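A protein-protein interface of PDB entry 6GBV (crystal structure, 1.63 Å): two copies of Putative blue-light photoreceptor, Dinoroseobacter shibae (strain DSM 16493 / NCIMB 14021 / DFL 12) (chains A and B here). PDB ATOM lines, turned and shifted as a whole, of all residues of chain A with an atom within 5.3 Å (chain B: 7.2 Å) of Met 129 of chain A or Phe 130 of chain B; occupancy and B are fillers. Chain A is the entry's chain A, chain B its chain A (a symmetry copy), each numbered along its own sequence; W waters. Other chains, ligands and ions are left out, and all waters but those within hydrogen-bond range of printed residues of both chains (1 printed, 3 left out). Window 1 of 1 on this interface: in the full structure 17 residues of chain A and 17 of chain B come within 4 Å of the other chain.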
ATOM      1  N   ALA A  22      -8.413  12.077 -15.805  1.00  0.00           N
ATOM      2  CA  ALA A  22      -7.306  12.746 -16.474  1.00  0.00           C
ATOM      3  C   ALA A  22      -6.253  11.728 -16.891  1.00  0.00           C
ATOM      4  O   ALA A  22      -5.904  10.821 -16.131  1.00  0.00           O
ATOM      5  CB  ALA A  22      -6.691  13.804 -15.556  1.00  0.00           C
ATOM      6  N   SER A  40       3.602  13.275  -8.299  1.00  0.00           N
ATOM      7  CA  SER A  40       3.137  13.770  -7.014  1.00  0.00           C
ATOM      8  C   SER A  40       2.495  15.138  -7.196  1.00  0.00           C
ATOM      9  O   SER A  40       2.760  15.843  -8.170  1.00  0.00           O
ATOM     10  CB  SER A  40       4.283  13.874  -6.003  1.00  0.00           C
ATOM     11  OG  SER A  40       5.072  15.028  -6.265  1.00  0.00           O
ATOM     12  N   ASP A  41       1.641  15.505  -6.238  1.00  0.00           N
ATOM     13  CA  ASP A  41       0.937  16.786  -6.240  1.00  0.00           C
ATOM     14  C   ASP A  41       1.450  17.643  -5.094  1.00  0.00           C
ATOM     15  O   ASP A  41       0.971  17.506  -3.956  1.00  0.00           O
ATOM     16  CB  ASP A  41      -0.572  16.567  -6.108  1.00  0.00           C
ATOM     17  CG  ASP A  41      -1.376  17.854  -6.278  1.00  0.00           C
ATOM     18  OD1 ASP A  41      -0.776  18.936  -6.434  1.00  0.00           O
ATOM     19  OD2 ASP A  41      -2.621  17.781  -6.254  1.00  0.00           O
ATOM     20  N   PRO A  42       2.405  18.546  -5.333  1.00  0.00           N
ATOM     21  CA  PRO A  42       2.951  19.356  -4.233  1.00  0.00           C
ATOM     22  C   PRO A  42       1.976  20.378  -3.668  1.00  0.00           C
ATOM     23  O   PRO A  42       2.282  20.983  -2.633  1.00  0.00           O
ATOM     24  CB  PRO A  42       4.167  20.040  -4.870  1.00  0.00           C
ATOM     25  CG  PRO A  42       3.858  20.064  -6.344  1.00  0.00           C
ATOM     26  CD  PRO A  42       3.083  18.802  -6.614  1.00  0.00           C
ATOM     27  N   SER A  43       0.827  20.601  -4.301  1.00  0.00           N
ATOM     28  CA  SER A  43      -0.167  21.503  -3.732  1.00  0.00           C
ATOM     29  C   SER A  43      -0.993  20.850  -2.633  1.00  0.00           C
ATOM     30  O   SER A  43      -1.713  21.556  -1.915  1.00  0.00           O
ATOM     31  CB  SER A  43      -1.094  22.027  -4.828  1.00  0.00           C
ATOM     32  OG  SER A  43      -2.092  21.076  -5.148  1.00  0.00           O
ATOM     33  N   ILE A 121       6.931  20.007 -13.067  1.00  0.00           N
ATOM     34  CA  ILE A 121       6.010  20.266 -14.168  1.00  0.00           C
ATOM     35  C   ILE A 121       5.154  21.469 -13.798  1.00  0.00           C
ATOM     36  O   ILE A 121       4.540  21.485 -12.726  1.00  0.00           O
ATOM     37  CB  ILE A 121       5.125  19.043 -14.463  1.00  0.00           C
ATOM     38  CG1 ILE A 121       5.982  17.827 -14.807  1.00  0.00           C
ATOM     39  CG2 ILE A 121       4.150  19.363 -15.595  1.00  0.00           C
ATOM     40  CD1 ILE A 121       5.170  16.616 -15.160  1.00  0.00           C
ATOM     41  N   TYR A 122       5.106  22.469 -14.679  1.00  0.00           N
ATOM     42  CA  TYR A 122       4.440  23.733 -14.402  1.00  0.00           C
ATOM     43  C   TYR A 122       3.134  23.851 -15.181  1.00  0.00           C
ATOM     44  O   TYR A 122       2.929  23.180 -16.194  1.00  0.00           O
ATOM     45  CB  TYR A 122       5.361  24.912 -14.750  1.00  0.00           C
ATOM     46  CG  TYR A 122       6.662  24.875 -13.989  1.00  0.00           C
ATOM     47  CD1 TYR A 122       7.757  24.163 -14.472  1.00  0.00           C
ATOM     48  CD2 TYR A 122       6.795  25.538 -12.776  1.00  0.00           C
ATOM     49  CE1 TYR A 122       8.951  24.119 -13.765  1.00  0.00           C
ATOM     50  CE2 TYR A 122       7.981  25.504 -12.068  1.00  0.00           C
ATOM     51  CZ  TYR A 122       9.052  24.795 -12.567  1.00  0.00           C
ATOM     52  OH  TYR A 122      10.221  24.760 -11.856  1.00  0.00           O
ATOM     53  N   ASP A 123       2.247  24.717 -14.694  1.00  0.00           N
ATOM     54  CA  ASP A 123       1.025  25.052 -15.418  1.00  0.00           C
ATOM     55  C   ASP A 123       1.276  26.253 -16.317  1.00  0.00           C
ATOM     56  O   ASP A 123       2.320  26.902 -16.213  1.00  0.00           O
ATOM     57  CB  ASP A 123      -0.131  25.276 -14.429  1.00  0.00           C
ATOM     58  CG  ASP A 123       0.017  26.528 -13.555  1.00  0.00           C
ATOM     59  OD1 ASP A 123       0.831  27.430 -13.846  1.00  0.00           O
ATOM     60  OD2 ASP A 123      -0.728  26.603 -12.548  1.00  0.00           O
ATOM     61  N   ASN A 127       3.064  28.381 -12.512  1.00  0.00           N
ATOM     62  CA  ASN A 127       3.058  27.849 -11.162  1.00  0.00           C
ATOM     63  C   ASN A 127       3.392  26.366 -11.198  1.00  0.00           C
ATOM     64  O   ASN A 127       2.996  25.648 -12.121  1.00  0.00           O
ATOM     65  CB  ASN A 127       1.693  28.054 -10.505  1.00  0.00           C
ATOM     66  CG  ASN A 127       1.286  29.507 -10.447  1.00  0.00           C
ATOM     67  OD1 ASN A 127       2.121  30.402 -10.573  1.00  0.00           O
ATOM     68  ND2 ASN A 127      -0.005  29.753 -10.248  1.00  0.00           N
ATOM     69  N   LEU A 128       4.135  25.918 -10.190  1.00  0.00           N
ATOM     70  CA  LEU A 128       4.406  24.495 -10.038  1.00  0.00           C
ATOM     71  C   LEU A 128       3.099  23.722  -9.936  1.00  0.00           C
ATOM     72  O   LEU A 128       2.172  24.120  -9.227  1.00  0.00           O
ATOM     73  CB  LEU A 128       5.263  24.256  -8.797  1.00  0.00           C
ATOM     74  CG  LEU A 128       5.625  22.807  -8.474  1.00  0.00           C
ATOM     75  CD1 LEU A 128       6.538  22.221  -9.542  1.00  0.00           C
ATOM     76  CD2 LEU A 128       6.262  22.719  -7.098  1.00  0.00           C
ATOM     77  N   MET A 129       3.028  22.612 -10.661  1.00  0.00           N
ATOM     78  CA  MET A 129       1.817  21.811 -10.729  1.00  0.00           C
ATOM     79  C   MET A 129       2.023  20.396 -10.212  1.00  0.00           C
ATOM     80  O   MET A 129       1.271  19.942  -9.339  1.00  0.00           O
ATOM     81  CB  MET A 129       1.321  21.786 -12.177  1.00  0.00           C
ATOM     82  CG  MET A 129      -0.151  21.579 -12.323  1.00  0.00           C
ATOM     83  SD  MET A 129      -0.606  21.737 -14.055  1.00  0.00           S
ATOM     84  CE  MET A 129      -2.358  21.398 -13.956  1.00  0.00           C
ATOM     85  N   PHE A 130       3.029  19.689 -10.726  1.00  0.00           N
ATOM     86  CA  PHE A 130       3.323  18.319 -10.331  1.00  0.00           C
ATOM     87  C   PHE A 130       4.825  18.140 -10.252  1.00  0.00           C
ATOM     88  O   PHE A 130       5.592  18.946 -10.782  1.00  0.00           O
ATOM     89  CB  PHE A 130       2.778  17.282 -11.325  1.00  0.00           C
ATOM     90  CG  PHE A 130       1.335  17.464 -11.668  1.00  0.00           C
ATOM     91  CD1 PHE A 130       0.350  17.075 -10.781  1.00  0.00           C
ATOM     92  CD2 PHE A 130       0.961  18.009 -12.886  1.00  0.00           C
ATOM     93  CE1 PHE A 130      -0.987  17.242 -11.092  1.00  0.00           C
ATOM     94  CE2 PHE A 130      -0.376  18.170 -13.209  1.00  0.00           C
ATOM     95  CZ  PHE A 130      -1.352  17.788 -12.306  1.00  0.00           C
ATOM     96  N   PHE A 131       5.237  17.057  -9.599  1.00  0.00           N
ATOM     97  CA  PHE A 131       6.568  16.503  -9.774  1.00  0.00           C
ATOM     98  C   PHE A 131       6.440  15.160 -10.480  1.00  0.00           C
ATOM     99  O   PHE A 131       5.517  14.384 -10.201  1.00  0.00           O
ATOM    100  CB  PHE A 131       7.292  16.318  -8.439  1.00  0.00           C
ATOM    101  CG  PHE A 131       7.792  17.599  -7.821  1.00  0.00           C
ATOM    102  CD1 PHE A 131       8.858  18.279  -8.381  1.00  0.00           C
ATOM    103  CD2 PHE A 131       7.207  18.108  -6.672  1.00  0.00           C
ATOM    104  CE1 PHE A 131       9.337  19.443  -7.803  1.00  0.00           C
ATOM    105  CE2 PHE A 131       7.685  19.272  -6.088  1.00  0.00           C
ATOM    106  CZ  PHE A 131       8.744  19.943  -6.660  1.00  0.00           C
ATOM    107  N   ILE B  21       6.163  22.364 -19.334  1.00  0.00           N
ATOM    108  CA  ILE B  21       4.810  22.851 -19.096  1.00  0.00           C
ATOM    109  C   ILE B  21       3.844  21.707 -19.361  1.00  0.00           C
ATOM    110  O   ILE B  21       3.947  21.025 -20.388  1.00  0.00           O
ATOM    111  CB  ILE B  21       4.484  24.060 -19.989  1.00  0.00           C
ATOM    112  CG1 ILE B  21       5.560  25.135 -19.851  1.00  0.00           C
ATOM    113  CG2 ILE B  21       3.118  24.631 -19.633  1.00  0.00           C
ATOM    114  CD1 ILE B  21       5.584  25.798 -18.498  1.00  0.00           C
ATOM    115  N   ALA B  22       2.914  21.488 -18.437  1.00  0.00           N
ATOM    116  CA  ALA B  22       1.916  20.447 -18.633  1.00  0.00           C
ATOM    117  C   ALA B  22       1.068  20.757 -19.860  1.00  0.00           C
ATOM    118  O   ALA B  22       0.652  21.898 -20.078  1.00  0.00           O
ATOM    119  CB  ALA B  22       1.030  20.319 -17.392  1.00  0.00           C
ATOM    120  N   ASP B  23       0.834  19.732 -20.681  1.00  0.00           N
ATOM    121  CA  ASP B  23      -0.023  19.852 -21.860  1.00  0.00           C
ATOM    122  C   ASP B  23      -1.468  19.638 -21.417  1.00  0.00           C
ATOM    123  O   ASP B  23      -2.029  18.543 -21.511  1.00  0.00           O
ATOM    124  CB  ASP B  23       0.391  18.849 -22.929  1.00  0.00           C
ATOM    125  CG  ASP B  23      -0.494  18.904 -24.158  1.00  0.00           C
ATOM    126  OD1 ASP B  23      -1.210  19.912 -24.340  1.00  0.00           O
ATOM    127  OD2 ASP B  23      -0.477  17.930 -24.943  1.00  0.00           O
ATOM    128  N   LEU B  24      -2.080  20.714 -20.918  1.00  0.00           N
ATOM    129  CA  LEU B  24      -3.431  20.595 -20.377  1.00  0.00           C
ATOM    130  C   LEU B  24      -4.439  20.228 -21.456  1.00  0.00           C
ATOM    131  O   LEU B  24      -5.441  19.565 -21.167  1.00  0.00           O
ATOM    132  CB  LEU B  24      -3.835  21.894 -19.682  1.00  0.00           C
ATOM    133  CG  LEU B  24      -3.009  22.236 -18.440  1.00  0.00           C
ATOM    134  CD1 LEU B  24      -3.600  23.425 -17.712  1.00  0.00           C
ATOM    135  CD2 LEU B  24      -2.909  21.034 -17.518  1.00  0.00           C
ATOM    136  N   LEU B  27      -6.255  16.794 -22.289  1.00  0.00           N
ATOM    137  CA  LEU B  27      -7.442  16.317 -21.601  1.00  0.00           C
ATOM    138  C   LEU B  27      -8.725  16.811 -22.250  1.00  0.00           C
ATOM    139  O   LEU B  27      -9.813  16.490 -21.762  1.00  0.00           O
ATOM    140  CB  LEU B  27      -7.412  16.742 -20.126  1.00  0.00           C
ATOM    141  CG  LEU B  27      -6.079  16.500 -19.413  1.00  0.00           C
ATOM    142  CD1 LEU B  27      -6.097  17.068 -17.999  1.00  0.00           C
ATOM    143  CD2 LEU B  27      -5.729  15.021 -19.391  1.00  0.00           C
ATOM    144  N   PHE B  39     -10.083  25.481 -18.540  1.00  0.00           N
ATOM    145  CA  PHE B  39      -9.959  24.555 -17.425  1.00  0.00           C
ATOM    146  C   PHE B  39      -9.778  25.369 -16.158  1.00  0.00           C
ATOM    147  O   PHE B  39      -9.038  26.358 -16.151  1.00  0.00           O
ATOM    148  CB  PHE B  39      -8.772  23.606 -17.586  1.00  0.00           C
ATOM    149  CG  PHE B  39      -8.802  22.816 -18.847  1.00  0.00           C
ATOM    150  CD1 PHE B  39      -9.963  22.207 -19.274  1.00  0.00           C
ATOM    151  CD2 PHE B  39      -7.669  22.705 -19.623  1.00  0.00           C
ATOM    152  CE1 PHE B  39      -9.981  21.485 -20.451  1.00  0.00           C
ATOM    153  CE2 PHE B  39      -7.683  21.983 -20.794  1.00  0.00           C
ATOM    154  CZ  PHE B  39      -8.836  21.375 -21.207  1.00  0.00           C
ATOM    155  N   SER B  40     -10.462  24.961 -15.096  1.00  0.00           N
ATOM    156  CA  SER B  40     -10.323  25.583 -13.790  1.00  0.00           C
ATOM    157  C   SER B  40      -9.782  24.565 -12.796  1.00  0.00           C
ATOM    158  O   SER B  40      -9.900  23.355 -12.994  1.00  0.00           O
ATOM    159  CB  SER B  40     -11.659  26.132 -13.282  1.00  0.00           C
ATOM    160  OG  SER B  40     -12.476  25.076 -12.794  1.00  0.00           O
ATOM    161  N   ASP B  41      -9.184  25.075 -11.717  1.00  0.00           N
ATOM    162  CA  ASP B  41      -8.613  24.251 -10.653  1.00  0.00           C
ATOM    163  C   ASP B  41      -9.429  24.435  -9.384  1.00  0.00           C
ATOM    164  O   ASP B  41      -9.188  25.388  -8.625  1.00  0.00           O
ATOM    165  CB  ASP B  41      -7.151  24.632 -10.407  1.00  0.00           C
ATOM    166  CG  ASP B  41      -6.449  23.694  -9.429  1.00  0.00           C
ATOM    167  OD1 ASP B  41      -7.098  22.779  -8.882  1.00  0.00           O
ATOM    168  OD2 ASP B  41      -5.235  23.873  -9.205  1.00  0.00           O
ATOM    169  N   PRO B  42     -10.391  23.552  -9.095  1.00  0.00           N
ATOM    170  CA  PRO B  42     -11.225  23.732  -7.896  1.00  0.00           C
ATOM    171  C   PRO B  42     -10.485  23.518  -6.584  1.00  0.00           C
ATOM    172  O   PRO B  42     -11.054  23.815  -5.525  1.00  0.00           O
ATOM    173  CB  PRO B  42     -12.338  22.694  -8.084  1.00  0.00           C
ATOM    174  CG  PRO B  42     -11.731  21.648  -8.982  1.00  0.00           C
ATOM    175  CD  PRO B  42     -10.806  22.396  -9.905  1.00  0.00           C
ATOM    176  N   SER B  43      -9.254  23.014  -6.605  1.00  0.00           N
ATOM    177  CA  SER B  43      -8.486  22.888  -5.372  1.00  0.00           C
ATOM    178  C   SER B  43      -7.853  24.202  -4.937  1.00  0.00           C
ATOM    179  O   SER B  43      -7.365  24.294  -3.803  1.00  0.00           O
ATOM    180  CB  SER B  43      -7.402  21.823  -5.532  1.00  0.00           C
ATOM    181  OG  SER B  43      -6.277  22.342  -6.218  1.00  0.00           O
ATOM    182  N   ASN B  47     -11.584  28.789  -7.412  1.00  0.00           N
ATOM    183  CA  ASN B  47     -11.711  27.986  -8.623  1.00  0.00           C
ATOM    184  C   ASN B  47     -11.178  28.718  -9.863  1.00  0.00           C
ATOM    185  O   ASN B  47     -11.917  28.933 -10.828  1.00  0.00           O
ATOM    186  CB  ASN B  47     -13.164  27.579  -8.819  1.00  0.00           C
ATOM    187  CG  ASN B  47     -13.341  26.519  -9.882  1.00  0.00           C
ATOM    188  OD1 ASN B  47     -12.441  25.720 -10.144  1.00  0.00           O
ATOM    189  ND2 ASN B  47     -14.508  26.512 -10.509  1.00  0.00           N
ATOM    190  N   ILE B  50      -6.895  27.851 -15.137  1.00  0.00           N
ATOM    191  CA  ILE B  50      -5.493  27.489 -15.309  1.00  0.00           C
ATOM    192  C   ILE B  50      -5.116  27.309 -16.764  1.00  0.00           C
ATOM    193  O   ILE B  50      -3.915  27.227 -17.070  1.00  0.00           O
ATOM    194  CB  ILE B  50      -5.135  26.218 -14.514  1.00  0.00           C
ATOM    195  CG1 ILE B  50      -6.062  25.068 -14.917  1.00  0.00           C
ATOM    196  CG2 ILE B  50      -5.206  26.500 -13.025  1.00  0.00           C
ATOM    197  CD1 ILE B  50      -5.538  23.719 -14.557  1.00  0.00           C
ATOM    198  N   ARG B 119     -17.807  19.934 -17.376  1.00  0.00           N
ATOM    199  CA  ARG B 119     -17.670  18.547 -16.965  1.00  0.00           C
ATOM    200  C   ARG B 119     -16.537  18.439 -15.954  1.00  0.00           C
ATOM    201  O   ARG B 119     -15.539  19.164 -16.060  1.00  0.00           O
ATOM    202  CB  ARG B 119     -17.395  17.631 -18.162  1.00  0.00           C
ATOM    203  CG  ARG B 119     -16.156  18.002 -18.937  1.00  0.00           C
ATOM    204  CD  ARG B 119     -16.040  17.220 -20.231  1.00  0.00           C
ATOM    205  NE  ARG B 119     -14.832  17.613 -20.946  1.00  0.00           N
ATOM    206  CZ  ARG B 119     -13.639  17.072 -20.731  1.00  0.00           C
ATOM    207  NH1 ARG B 119     -13.510  16.109 -19.827  1.00  0.00           N
ATOM    208  NH2 ARG B 119     -12.578  17.493 -21.411  1.00  0.00           N
ATOM    209  N   PRO B 120     -16.675  17.575 -14.957  1.00  0.00           N
ATOM    210  CA  PRO B 120     -15.586  17.375 -14.003  1.00  0.00           C
ATOM    211  C   PRO B 120     -14.565  16.396 -14.550  1.00  0.00           C
ATOM    212  O   PRO B 120     -14.892  15.488 -15.318  1.00  0.00           O
ATOM    213  CB  PRO B 120     -16.302  16.798 -12.779  1.00  0.00           C
ATOM    214  CG  PRO B 120     -17.438  16.032 -13.381  1.00  0.00           C
ATOM    215  CD  PRO B 120     -17.880  16.804 -14.593  1.00  0.00           C
ATOM    216  N   ILE B 121     -13.313  16.590 -14.136  1.00  0.00           N
ATOM    217  CA  ILE B 121     -12.210  15.704 -14.490  1.00  0.00           C
ATOM    218  C   ILE B 121     -11.562  15.215 -13.202  1.00  0.00           C
ATOM    219  O   ILE B 121     -11.190  16.028 -12.350  1.00  0.00           O
ATOM    220  CB  ILE B 121     -11.176  16.418 -15.378  1.00  0.00           C
ATOM    221  CG1 ILE B 121     -11.830  16.935 -16.658  1.00  0.00           C
ATOM    222  CG2 ILE B 121     -10.019  15.472 -15.698  1.00  0.00           C
ATOM    223  CD1 ILE B 121     -10.856  17.592 -17.591  1.00  0.00           C
ATOM    224  N   TYR B 122     -11.421  13.897 -13.061  1.00  0.00           N
ATOM    225  CA  TYR B 122     -10.944  13.282 -11.831  1.00  0.00           C
ATOM    226  C   TYR B 122      -9.520  12.759 -11.992  1.00  0.00           C
ATOM    227  O   TYR B 122      -9.048  12.515 -13.104  1.00  0.00           O
ATOM    228  CB  TYR B 122     -11.874  12.135 -11.410  1.00  0.00           C
ATOM    229  CG  TYR B 122     -13.297  12.588 -11.202  1.00  0.00           C
ATOM    230  CD1 TYR B 122     -14.198  12.636 -12.263  1.00  0.00           C
ATOM    231  CD2 TYR B 122     -13.740  12.988  -9.948  1.00  0.00           C
ATOM    232  CE1 TYR B 122     -15.505  13.065 -12.073  1.00  0.00           C
ATOM    233  CE2 TYR B 122     -15.039  13.412  -9.749  1.00  0.00           C
ATOM    234  CZ  TYR B 122     -15.915  13.448 -10.814  1.00  0.00           C
ATOM    235  OH  TYR B 122     -17.198  13.877 -10.610  1.00  0.00           O
ATOM    236  N   ASP B 123      -8.836  12.590 -10.862  1.00  0.00           N
ATOM    237  CA  ASP B 123      -7.525  11.949 -10.848  1.00  0.00           C
ATOM    238  C   ASP B 123      -7.690  10.452 -10.637  1.00  0.00           C
ATOM    239  O   ASP B 123      -8.786   9.983 -10.320  1.00  0.00           O
ATOM    240  CB  ASP B 123      -6.626  12.607  -9.788  1.00  0.00           C
ATOM    241  CG  ASP B 123      -7.066  12.355  -8.340  1.00  0.00           C
ATOM    242  OD1 ASP B 123      -7.878  11.449  -8.057  1.00  0.00           O
ATOM    243  OD2 ASP B 123      -6.557  13.092  -7.462  1.00  0.00           O
ATOM    244  N   ASN B 127     -10.418  11.548  -6.955  1.00  0.00           N
ATOM    245  CA  ASN B 127     -10.646  12.884  -6.437  1.00  0.00           C
ATOM    246  C   ASN B 127     -10.830  13.853  -7.594  1.00  0.00           C
ATOM    247  O   ASN B 127     -10.187  13.723  -8.639  1.00  0.00           O
ATOM    248  CB  ASN B 127      -9.472  13.336  -5.567  1.00  0.00           C
ATOM    249  CG  ASN B 127      -9.219  12.410  -4.402  1.00  0.00           C
ATOM    250  OD1 ASN B 127     -10.086  11.626  -4.019  1.00  0.00           O
ATOM    251  ND2 ASN B 127      -8.025  12.499  -3.824  1.00  0.00           N
ATOM    252  N   LEU B 128     -11.724  14.819  -7.400  1.00  0.00           N
ATOM    253  CA  LEU B 128     -11.891  15.887  -8.376  1.00  0.00           C
ATOM    254  C   LEU B 128     -10.570  16.612  -8.589  1.00  0.00           C
ATOM    255  O   LEU B 128      -9.851  16.929  -7.639  1.00  0.00           O
ATOM    256  CB  LEU B 128     -12.963  16.865  -7.901  1.00  0.00           C
ATOM    257  CG  LEU B 128     -13.253  18.065  -8.801  1.00  0.00           C
ATOM    258  CD1 LEU B 128     -13.866  17.623 -10.122  1.00  0.00           C
ATOM    259  CD2 LEU B 128     -14.153  19.055  -8.082  1.00  0.00           C
ATOM    260  N   MET B 129     -10.250  16.866  -9.853  1.00  0.00           N
ATOM    261  CA  MET B 129      -8.985  17.479 -10.219  1.00  0.00           C
ATOM    262  C   MET B 129      -9.166  18.809 -10.933  1.00  0.00           C
ATOM    263  O   MET B 129      -8.575  19.817 -10.521  1.00  0.00           O
ATOM    264  CB  MET B 129      -8.197  16.504 -11.096  1.00  0.00           C
ATOM    265  CG  MET B 129      -6.714  16.675 -11.034  1.00  0.00           C
ATOM    266  SD  MET B 129      -5.923  15.364 -11.977  1.00  0.00           S
ATOM    267  CE  MET B 129      -4.208  15.827 -11.789  1.00  0.00           C
ATOM    268  N   PHE B 130      -9.974  18.840 -11.992  1.00  0.00           N
ATOM    269  CA  PHE B 130     -10.220  20.043 -12.773  1.00  0.00           C
ATOM    270  C   PHE B 130     -11.683  20.089 -13.163  1.00  0.00           C
ATOM    271  O   PHE B 130     -12.391  19.083 -13.097  1.00  0.00           O
ATOM    272  CB  PHE B 130      -9.388  20.096 -14.064  1.00  0.00           C
ATOM    273  CG  PHE B 130      -7.928  19.854 -13.860  1.00  0.00           C
ATOM    274  CD1 PHE B 130      -7.118  20.848 -13.343  1.00  0.00           C
ATOM    275  CD2 PHE B 130      -7.358  18.638 -14.201  1.00  0.00           C
ATOM    276  CE1 PHE B 130      -5.767  20.630 -13.150  1.00  0.00           C
ATOM    277  CE2 PHE B 130      -6.003  18.415 -14.020  1.00  0.00           C
ATOM    278  CZ  PHE B 130      -5.207  19.414 -13.490  1.00  0.00           C
ATOM    279  N   PHE B 131     -12.123  21.268 -13.590  1.00  0.00           N
ATOM    280  CA  PHE B 131     -13.333  21.406 -14.382  1.00  0.00           C
ATOM    281  C   PHE B 131     -12.939  21.839 -15.789  1.00  0.00           C
ATOM    282  O   PHE B 131     -12.029  22.659 -15.966  1.00  0.00           O
ATOM    283  CB  PHE B 131     -14.300  22.426 -13.779  1.00  0.00           C
ATOM    284  CG  PHE B 131     -15.032  21.939 -12.554  1.00  0.00           C
ATOM    285  CD1 PHE B 131     -16.013  20.971 -12.661  1.00  0.00           C
ATOM    286  CD2 PHE B 131     -14.747  22.463 -11.303  1.00  0.00           C
ATOM    287  CE1 PHE B 131     -16.706  20.537 -11.543  1.00  0.00           C
ATOM    288  CE2 PHE B 131     -15.439  22.034 -10.179  1.00  0.00           C
ATOM    289  CZ  PHE B 131     -16.412  21.065 -10.299  1.00  0.00           C
ATOM    290  N   ALA B 132     -13.599  21.270 -16.788  1.00  0.00           N
ATOM    291  CA  ALA B 132     -13.473  21.725 -18.163  1.00  0.00           C
ATOM    292  C   ALA B 132     -14.768  22.405 -18.554  1.00  0.00           C
ATOM    293  O   ALA B 132     -15.847  21.852 -18.325  1.00  0.00           O
ATOM    294  CB  ALA B 132     -13.180  20.570 -19.120  1.00  0.00           C
HETATM  295  O   HOH W   1      -2.099  28.214 -15.357  1.00  0.00           O
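N of Ala 22 of chain A sits at hydrogen-bond distance from O of Tyr 122 of chain B (2.8 Å).
O of Tyr 122 of chain A sits at hydrogen-bond distance from N of Ala 22 of chain B (2.8 Å).
The backbone carbonyl oxygen (O) of Phe 130 of chain B is in hydrogen-bond range of the backbone NH (N) of Ile 121 of chain B (2.9 Å).
O of Ile 121 of chain A is in hydrogen-bond range of N of Met 129 of chain A, 2.8 Å away.
The backbone carbonyl oxygen of Phe 130 of chain A sits at hydrogen-bond distance from the backbone NH of Ile 121 of chain A, 2.9 Å away.
The backbone NH (N) of Ile 50 of chain B sits at hydrogen-bond distance from the backbone carbonyl oxygen (O) of Phe 39 of chain B, 2.8 Å away.
The backbone carbonyl oxygen (O) of Ile 121 of chain B lies within hydrogen-bond range of the backbone NH (N) of Met 129 of chain B, at 2.8 Å.
Among the printed residues, pairs that only touch across the chains: Tyr 122 of chain A with Ile 21 of chain B (3.5 Å), Phe 130 of chain A with Met 129 of chain B (3.5 Å), Met 129 of chain A with Phe 130 of chain B (3.5 Å), Met 129 of chain A with Leu 24 of chain B (3.6 Å), Ile 121 of chain A with Ala 22 of chain B (3.7 Å), Ala 22 of chain A with Ile 121 of chain B (3.7 Å), Met 129 of chain A with Ala 22 of chain B (3.98 Å), Ala 22 of chain A with Met 129 of chain B (3.98 Å) and Met 129 of chain A with Ile 50 of chain B (3.98 Å).
Of the printed residues of chain B, Met 129 of chain A touches Ala 22 (3.98 Å), Leu 24 (3.6 Å), Ile 50 (3.98 Å) and Phe 130 (3.5 Å).
Phe 130 of chain B touches one residue of chain A.
Of the printed residues of chain A, Met 129 of chain B touches Ala 22 and Phe 130.
Printed residues of chain A within 4 Å of Ala 22 of chain B: Ile 121, Tyr 122 and Met 129.
Of the printed residues of chain B, Tyr 122 of chain A touches Ile 21 (3.5 Å) and Ala 22 (2.8 Å).
Of the printed residues of chain A, Ile 50 of chain B touches Met 129 (3.98 Å).
Printed residues of chain A within 4 Å of Leu 24 of chain B: Met 129 (3.6 Å).
Ser 40 of chain B touches none of the printed residues of chain A.
Ala 132 of chain B touches none of the printed residues of chain A.
The nearest printed residue of chain B that does not touch Met 129 of chain A is Asp 41 of chain B (6.1 Å).
The nearest residue of chain A that does not touch Phe 130 of chain B is Phe 130 of chain A (4.3 Å).
The nearest printed residue of chain A that does not touch Met 129 of chain B is Asp 41 of chain A (6.1 Å).
Of the 23 printed residues of chain B, 8 touch a printed residue of chain A.
Among the printed residues, 11 pairs touch across the chains.
Among the printed residues, no Asp or Glu carboxylate lies within 4 Å of a Lys or Arg side-chain nitrogen of the other chain.
Ala 22 of chain A touches Ile 121 of chain B, and with the chains exchanged Ile 121 of chain A touches Ala 22 of chain B.
Ala 22 of chain A touches Tyr 122 of chain B, and with the chains exchanged Tyr 122 of chain A touches Ala 22 of chain B.
Ala 22 of chain A touches Met 129 of chain B, and with the chains exchanged Met 129 of chain A touches Ala 22 of chain B.
Met 129 of chain A touches Phe 130 of chain B, and with the chains exchanged Phe 130 of chain A touches Met 129 of chain B.
Positions printed for both chains: 22, 40, 41, 42, 43, 121, 122, 123, 127, 128, 129, 130 and 131.
Of the 11 pairs that touch across the chains among the printed residues, 8 have their exchanged pair printed and touching as well.
Water W1 lies within hydrogen-bond range of the backbone carbonyl oxygen (O) of Ile 50 of chain B and the side-chain carboxylate (OD1) of Asp 123 of chain A.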
